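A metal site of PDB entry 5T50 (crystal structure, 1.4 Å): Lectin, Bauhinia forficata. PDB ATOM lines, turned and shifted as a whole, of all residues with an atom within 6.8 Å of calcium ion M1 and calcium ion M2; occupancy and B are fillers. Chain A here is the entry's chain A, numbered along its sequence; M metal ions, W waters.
The backbone carbonyl oxygen (O) of Gly 136 is in hydrogen-bond range of the backbone NH (N) of Glu 118 (2.8 Å).
The side-chain carboxylate (OE1) of Glu 118 sits close to the side-chain carboxylate (OD2) of Asp 138 (2.5 Å).
The side-chain carboxylate of Glu 129 lies close to the indole nitrogen of Trp 127, 3.1 Å away.
Within 4 Å of calcium ion M1: Asp 120, Trp 122, Asn 124 and Glu 129.
The nearest printed residue that does not touch calcium ion M1 is Val 123 (4.5 Å).
Of the 22 residues printed, 4 come within 4 Å of calcium ion M2.
Calcium ion M1 is bound by the backbone carbonyl oxygen (O) of Trp 122 (2.3 Å), the side-chain amide oxygen (OD1) of Asn 124 (2.4 Å), water W2 (2.4 Å), water W4 (2.4 Å), the side-chain carboxylate (OD2) of Asp 120 (2.4 Å), the side-chain carboxylate (OE2) of Glu 129 (2.5 Å) and the side-chain carboxylate (OD1) of Asp 120 (2.5 Å).
Calcium ion M1 has seven donor atoms within binding distance.
Calcium ion M2 is bound by the side-chain carboxylate of Asp 120 (2.2 Å), the side-chain carboxylate of Glu 118 (2.2 Å), the side-chain carboxylate of Glu 129 (2.3 Å), water W1 (2.3 Å), water W3 (2.3 Å) and a ring nitrogen (NE2) of His 134 (2.5 Å).
Calcium ion M2 has six donor atoms within binding distance.
Water W3 lies within hydrogen-bond range of OE1 of Glu 118 (2.7 Å) and O of Ile 142 (2.8 Å).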
ATOM      1  N   ASP A  78     -21.193   2.657 -10.083  1.00  0.00           N
ATOM      2  CA  ASP A  78     -21.966   1.468  -9.688  1.00  0.00           C
ATOM      3  C   ASP A  78     -22.679   0.742 -10.823  1.00  0.00           C
ATOM      4  O   ASP A  78     -23.087  -0.401 -10.657  1.00  0.00           O
ATOM      5  CB  ASP A  78     -23.031   1.898  -8.674  1.00  0.00           C
ATOM      6  CG  ASP A  78     -22.479   1.906  -7.288  1.00  0.00           C
ATOM      7  OD1 ASP A  78     -22.445   0.840  -6.663  1.00  0.00           O
ATOM      8  OD2 ASP A  78     -21.997   3.000  -6.868  1.00  0.00           O
ATOM      9  N   GLY A  95     -24.978   5.539  -5.606  1.00  0.00           N
ATOM     10  CA  GLY A  95     -24.317   4.304  -5.257  1.00  0.00           C
ATOM     11  C   GLY A  95     -25.011   3.049  -5.748  1.00  0.00           C
ATOM     12  O   GLY A  95     -25.639   3.068  -6.838  1.00  0.00           O
ATOM     13  N   GLY A  96     -25.043   1.989  -4.929  1.00  0.00           N
ATOM     14  CA  GLY A  96     -25.550   0.690  -5.398  1.00  0.00           C
ATOM     15  C   GLY A  96     -27.049   0.657  -5.624  1.00  0.00           C
ATOM     16  O   GLY A  96     -27.581  -0.279  -6.248  1.00  0.00           O
ATOM     17  N   TYR A  97     -27.789   1.692  -5.147  1.00  0.00           N
ATOM     18  CA  TYR A  97     -29.195   1.819  -5.441  1.00  0.00           C
ATOM     19  C   TYR A  97     -29.484   2.188  -6.887  1.00  0.00           C
ATOM     20  O   TYR A  97     -30.666   2.186  -7.280  1.00  0.00           O
ATOM     21  CB  TYR A  97     -29.828   2.800  -4.469  1.00  0.00           C
ATOM     22  CG  TYR A  97     -29.681   2.364  -3.037  1.00  0.00           C
ATOM     23  CD1 TYR A  97     -30.430   1.361  -2.492  1.00  0.00           C
ATOM     24  CD2 TYR A  97     -28.691   2.952  -2.220  1.00  0.00           C
ATOM     25  CE1 TYR A  97     -30.211   0.954  -1.153  1.00  0.00           C
ATOM     26  CE2 TYR A  97     -28.473   2.543  -0.904  1.00  0.00           C
ATOM     27  CZ  TYR A  97     -29.258   1.518  -0.384  1.00  0.00           C
ATOM     28  OH  TYR A  97     -29.054   1.127   0.954  1.00  0.00           O
ATOM     29  N   LEU A  98     -28.435   2.597  -7.633  1.00  0.00           N
ATOM     30  CA  LEU A  98     -28.535   2.828  -9.081  1.00  0.00           C
ATOM     31  C   LEU A  98     -29.474   3.914  -9.506  1.00  0.00           C
ATOM     32  O   LEU A  98     -29.909   4.013 -10.630  1.00  0.00           O
ATOM     33  CB  LEU A  98     -28.792   1.500  -9.837  1.00  0.00           C
ATOM     34  CG  LEU A  98     -27.770   0.388  -9.754  1.00  0.00           C
ATOM     35  CD1 LEU A  98     -28.260  -0.851 -10.475  1.00  0.00           C
ATOM     36  CD2 LEU A  98     -26.475   0.876 -10.413  1.00  0.00           C
ATOM     37  N   GLU A 118     -30.516  -4.044 -15.348  1.00  0.00           N
ATOM     38  CA  GLU A 118     -29.370  -3.386 -14.756  1.00  0.00           C
ATOM     39  C   GLU A 118     -28.042  -3.982 -15.243  1.00  0.00           C
ATOM     40  O   GLU A 118     -27.948  -5.187 -15.533  1.00  0.00           O
ATOM     41  CB  GLU A 118     -29.390  -3.437 -13.212  1.00  0.00           C
ATOM     42  CG  GLU A 118     -29.341  -4.845 -12.641  1.00  0.00           C
ATOM     43  CD  GLU A 118     -29.022  -4.803 -11.148  1.00  0.00           C
ATOM     44  OE1 GLU A 118     -29.843  -4.104 -10.413  1.00  0.00           O
ATOM     45  OE2 GLU A 118     -28.079  -5.527 -10.708  1.00  0.00           O
ATOM     46  N   ASP A 120     -24.471  -3.991 -13.669  1.00  0.00           N
ATOM     47  CA  ASP A 120     -24.029  -3.734 -12.274  1.00  0.00           C
ATOM     48  C   ASP A 120     -22.524  -3.984 -12.201  1.00  0.00           C
ATOM     49  O   ASP A 120     -22.071  -5.135 -12.289  1.00  0.00           O
ATOM     50  CB  ASP A 120     -24.811  -4.592 -11.314  1.00  0.00           C
ATOM     51  CG  ASP A 120     -24.576  -4.184  -9.858  1.00  0.00           C
ATOM     52  OD1 ASP A 120     -23.565  -3.556  -9.571  1.00  0.00           O
ATOM     53  OD2 ASP A 120     -25.459  -4.512  -9.007  1.00  0.00           O
ATOM     54  N   THR A 121     -21.755  -2.897 -12.044  1.00  0.00           N
ATOM     55  CA  THR A 121     -20.280  -3.007 -11.977  1.00  0.00           C
ATOM     56  C   THR A 121     -19.660  -3.186 -10.631  1.00  0.00           C
ATOM     57  O   THR A 121     -18.443  -3.348 -10.540  1.00  0.00           O
ATOM     58  CB  THR A 121     -19.629  -1.720 -12.627  1.00  0.00           C
ATOM     59  OG1 THR A 121     -20.068  -0.615 -11.836  1.00  0.00           O
ATOM     60  CG2 THR A 121     -20.033  -1.554 -14.072  1.00  0.00           C
ATOM     61  N   TRP A 122     -20.486  -3.146  -9.577  1.00  0.00           N
ATOM     62  CA  TRP A 122     -19.967  -3.102  -8.206  1.00  0.00           C
ATOM     63  C   TRP A 122     -20.762  -4.060  -7.319  1.00  0.00           C
ATOM     64  O   TRP A 122     -21.966  -3.977  -7.161  1.00  0.00           O
ATOM     65  CB  TRP A 122     -20.069  -1.690  -7.637  1.00  0.00           C
ATOM     66  CG  TRP A 122     -19.647  -1.619  -6.194  1.00  0.00           C
ATOM     67  CD1 TRP A 122     -20.444  -1.811  -5.149  1.00  0.00           C
ATOM     68  CD2 TRP A 122     -18.333  -1.374  -5.690  1.00  0.00           C
ATOM     69  NE1 TRP A 122     -19.737  -1.666  -3.962  1.00  0.00           N
ATOM     70  CE2 TRP A 122     -18.413  -1.431  -4.265  1.00  0.00           C
ATOM     71  CE3 TRP A 122     -17.096  -1.070  -6.271  1.00  0.00           C
ATOM     72  CZ2 TRP A 122     -17.307  -1.188  -3.446  1.00  0.00           C
ATOM     73  CZ3 TRP A 122     -16.009  -0.840  -5.486  1.00  0.00           C
ATOM     74  CH2 TRP A 122     -16.135  -0.890  -4.056  1.00  0.00           C
ATOM     75  N   VAL A 123     -20.059  -5.030  -6.759  1.00  0.00           N
ATOM     76  CA  VAL A 123     -20.680  -6.039  -5.907  1.00  0.00           C
ATOM     77  C   VAL A 123     -20.969  -5.406  -4.538  1.00  0.00           C
ATOM     78  O   VAL A 123     -20.066  -5.031  -3.787  1.00  0.00           O
ATOM     79  CB  VAL A 123     -19.753  -7.277  -5.748  1.00  0.00           C
ATOM     80  CG1 VAL A 123     -20.315  -8.190  -4.659  1.00  0.00           C
ATOM     81  CG2 VAL A 123     -19.521  -7.965  -7.098  1.00  0.00           C
ATOM     82  N   ASN A 124     -22.275  -5.328  -4.238  1.00  0.00           N
ATOM     83  CA  ASN A 124     -22.753  -4.777  -2.947  1.00  0.00           C
ATOM     84  C   ASN A 124     -22.893  -5.889  -1.920  1.00  0.00           C
ATOM     85  O   ASN A 124     -23.437  -6.951  -2.282  1.00  0.00           O
ATOM     86  CB  ASN A 124     -24.065  -4.058  -3.122  1.00  0.00           C
ATOM     87  CG  ASN A 124     -23.834  -2.708  -3.808  1.00  0.00           C
ATOM     88  OD1 ASN A 124     -23.945  -2.563  -5.024  1.00  0.00           O
ATOM     89  ND2 ASN A 124     -23.437  -1.718  -2.987  1.00  0.00           N
ATOM     90  N   TRP A 127     -27.064  -5.953   0.406  1.00  0.00           N
ATOM     91  CA  TRP A 127     -28.184  -6.802   0.027  1.00  0.00           C
ATOM     92  C   TRP A 127     -27.578  -7.972  -0.728  1.00  0.00           C
ATOM     93  O   TRP A 127     -26.384  -7.913  -1.080  1.00  0.00           O
ATOM     94  CB  TRP A 127     -29.208  -6.061  -0.826  1.00  0.00           C
ATOM     95  CG  TRP A 127     -28.649  -5.332  -1.967  1.00  0.00           C
ATOM     96  CD1 TRP A 127     -28.364  -5.815  -3.259  1.00  0.00           C
ATOM     97  CD2 TRP A 127     -28.287  -3.953  -1.994  1.00  0.00           C
ATOM     98  NE1 TRP A 127     -27.800  -4.818  -3.973  1.00  0.00           N
ATOM     99  CE2 TRP A 127     -27.714  -3.666  -3.257  1.00  0.00           C
ATOM    100  CE3 TRP A 127     -28.308  -2.941  -1.039  1.00  0.00           C
ATOM    101  CZ2 TRP A 127     -27.292  -2.389  -3.596  1.00  0.00           C
ATOM    102  CZ3 TRP A 127     -27.812  -1.689  -1.378  1.00  0.00           C
ATOM    103  CH2 TRP A 127     -27.309  -1.429  -2.651  1.00  0.00           C
ATOM    104  N   LYS A 128     -28.429  -8.930  -1.109  1.00  0.00           N
ATOM    105  CA  LYS A 128     -27.925 -10.087  -1.844  1.00  0.00           C
ATOM    106  C   LYS A 128     -27.732  -9.844  -3.309  1.00  0.00           C
ATOM    107  O   LYS A 128     -28.692  -9.447  -3.991  1.00  0.00           O
ATOM    108  CB  LYS A 128     -28.920 -11.220  -1.718  1.00  0.00           C
ATOM    109  CG  LYS A 128     -28.899 -11.792  -0.330  1.00  0.00           C
ATOM    110  CD  LYS A 128     -27.829 -12.851  -0.094  1.00  0.00           C
ATOM    111  CE  LYS A 128     -28.018 -13.522   1.262  1.00  0.00           C
ATOM    112  NZ  LYS A 128     -26.699 -13.960   1.835  1.00  0.00           N
ATOM    113  N   GLU A 129     -26.502  -9.973  -3.746  1.00  0.00           N
ATOM    114  CA  GLU A 129     -26.212 -10.065  -5.173  1.00  0.00           C
ATOM    115  C   GLU A 129     -25.002 -10.912  -5.430  1.00  0.00           C
ATOM    116  O   GLU A 129     -24.287 -11.277  -4.507  1.00  0.00           O
ATOM    117  CB  GLU A 129     -26.191  -8.712  -5.800  1.00  0.00           C
ATOM    118  CG  GLU A 129     -25.149  -7.767  -5.342  1.00  0.00           C
ATOM    119  CD  GLU A 129     -25.341  -6.359  -6.027  1.00  0.00           C
ATOM    120  OE1 GLU A 129     -26.476  -5.988  -6.545  1.00  0.00           O
ATOM    121  OE2 GLU A 129     -24.305  -5.666  -6.118  1.00  0.00           O
ATOM    122  N   PRO A 130     -24.799 -11.300  -6.723  1.00  0.00           N
ATOM    123  CA  PRO A 130     -23.665 -12.155  -7.000  1.00  0.00           C
ATOM    124  C   PRO A 130     -22.322 -11.564  -6.637  1.00  0.00           C
ATOM    125  O   PRO A 130     -22.193 -10.348  -6.568  1.00  0.00           O
ATOM    126  CB  PRO A 130     -23.765 -12.329  -8.523  1.00  0.00           C
ATOM    127  CG  PRO A 130     -25.134 -11.994  -8.902  1.00  0.00           C
ATOM    128  CD  PRO A 130     -25.622 -11.022  -7.892  1.00  0.00           C
ATOM    129  N   HIS A 134     -22.416  -8.204 -12.923  1.00  0.00           N
ATOM    130  CA  HIS A 134     -23.595  -8.922 -13.428  1.00  0.00           C
ATOM    131  C   HIS A 134     -24.576  -8.014 -14.115  1.00  0.00           C
ATOM    132  O   HIS A 134     -24.590  -6.802 -13.895  1.00  0.00           O
ATOM    133  CB  HIS A 134     -24.279  -9.687 -12.262  1.00  0.00           C
ATOM    134  CG  HIS A 134     -24.631  -8.836 -11.084  1.00  0.00           C
ATOM    135  ND1 HIS A 134     -23.714  -8.559 -10.111  1.00  0.00           N
ATOM    136  CD2 HIS A 134     -25.758  -8.168 -10.752  1.00  0.00           C
ATOM    137  CE1 HIS A 134     -24.268  -7.754  -9.238  1.00  0.00           C
ATOM    138  NE2 HIS A 134     -25.491  -7.522  -9.581  1.00  0.00           N
ATOM    139  N   GLY A 136     -28.766  -7.925 -14.737  1.00  0.00           N
ATOM    140  CA  GLY A 136     -29.941  -8.444 -14.083  1.00  0.00           C
ATOM    141  C   GLY A 136     -31.227  -7.843 -14.504  1.00  0.00           C
ATOM    142  O   GLY A 136     -31.257  -6.724 -15.025  1.00  0.00           O
ATOM    143  N   ASP A 138     -34.624  -6.533 -12.683  1.00  0.00           N
ATOM    144  CA  ASP A 138     -35.087  -6.105 -11.386  1.00  0.00           C
ATOM    145  C   ASP A 138     -36.582  -5.842 -11.497  1.00  0.00           C
ATOM    146  O   ASP A 138     -37.033  -5.105 -12.385  1.00  0.00           O
ATOM    147  CB  ASP A 138     -34.383  -4.808 -10.958  1.00  0.00           C
ATOM    148  CG  ASP A 138     -32.916  -4.915 -10.814  1.00  0.00           C
ATOM    149  OD1 ASP A 138     -32.408  -6.019 -10.723  1.00  0.00           O
ATOM    150  OD2 ASP A 138     -32.246  -3.843 -10.842  1.00  0.00           O
ATOM    151  N   ILE A 142     -34.033  -3.983  -5.621  1.00  0.00           N
ATOM    152  CA  ILE A 142     -32.620  -3.966  -6.011  1.00  0.00           C
ATOM    153  C   ILE A 142     -31.975  -5.346  -6.058  1.00  0.00           C
ATOM    154  O   ILE A 142     -30.884  -5.500  -6.642  1.00  0.00           O
ATOM    155  CB  ILE A 142     -31.837  -2.994  -5.096  1.00  0.00           C
ATOM    156  CG1 ILE A 142     -30.490  -2.511  -5.680  1.00  0.00           C
ATOM    157  CG2 ILE A 142     -31.708  -3.625  -3.669  1.00  0.00           C
ATOM    158  CD1 ILE A 142     -30.593  -1.832  -7.075  1.00  0.00           C
ATOM    159  N   VAL A 143     -32.661  -6.359  -5.501  1.00  0.00           N
ATOM    160  CA  VAL A 143     -32.209  -7.748  -5.547  1.00  0.00           C
ATOM    161  C   VAL A 143     -32.843  -8.335  -6.825  1.00  0.00           C
ATOM    162  O   VAL A 143     -34.049  -8.550  -6.908  1.00  0.00           O
ATOM    163  CB  VAL A 143     -32.599  -8.517  -4.276  1.00  0.00           C
ATOM    164  CG1 VAL A 143     -32.227  -9.995  -4.443  1.00  0.00           C
ATOM    165  CG2 VAL A 143     -31.901  -7.978  -3.058  1.00  0.00           C
ATOM    166  N   SER A 144     -32.016  -8.567  -7.823  1.00  0.00           N
ATOM    167  CA  SER A 144     -32.488  -9.037  -9.106  1.00  0.00           C
ATOM    168  C   SER A 144     -33.203 -10.371  -9.016  1.00  0.00           C
ATOM    169  O   SER A 144     -32.737 -11.288  -8.360  1.00  0.00           O
ATOM    170  CB  SER A 144     -31.313  -9.135 -10.114  1.00  0.00           C
ATOM    171  OG  SER A 144     -30.619  -7.906 -10.277  1.00  0.00           O
ATOM    172  N   VAL A 147     -30.425 -13.014 -12.921  1.00  0.00           N
ATOM    173  CA  VAL A 147     -29.137 -12.329 -12.964  1.00  0.00           C
ATOM    174  C   VAL A 147     -28.159 -13.273 -13.616  1.00  0.00           C
ATOM    175  O   VAL A 147     -28.284 -14.514 -13.475  1.00  0.00           O
ATOM    176  CB  VAL A 147     -28.736 -11.922 -11.468  1.00  0.00           C
ATOM    177  CG1 VAL A 147     -28.401 -13.138 -10.609  1.00  0.00           C
ATOM    178  CG2 VAL A 147     -27.721 -10.868 -11.412  1.00  0.00           C
HETATM  179 CA    CA M   1     -24.238  -3.439  -7.185  1.00  0.00          CA
HETATM  180 CA    CA M   2     -27.153  -5.939  -8.709  1.00  0.00          CA
HETATM  181  O   HOH W   1     -28.543  -7.749  -8.608  1.00  0.00           O
HETATM  182  O   HOH W   2     -23.747  -1.217  -7.899  1.00  0.00           O
HETATM  183  O   HOH W   3     -28.721  -4.370  -7.950  1.00  0.00           O
HETATM  184  O   HOH W   4     -26.532  -2.669  -6.981  1.00  0.00           O
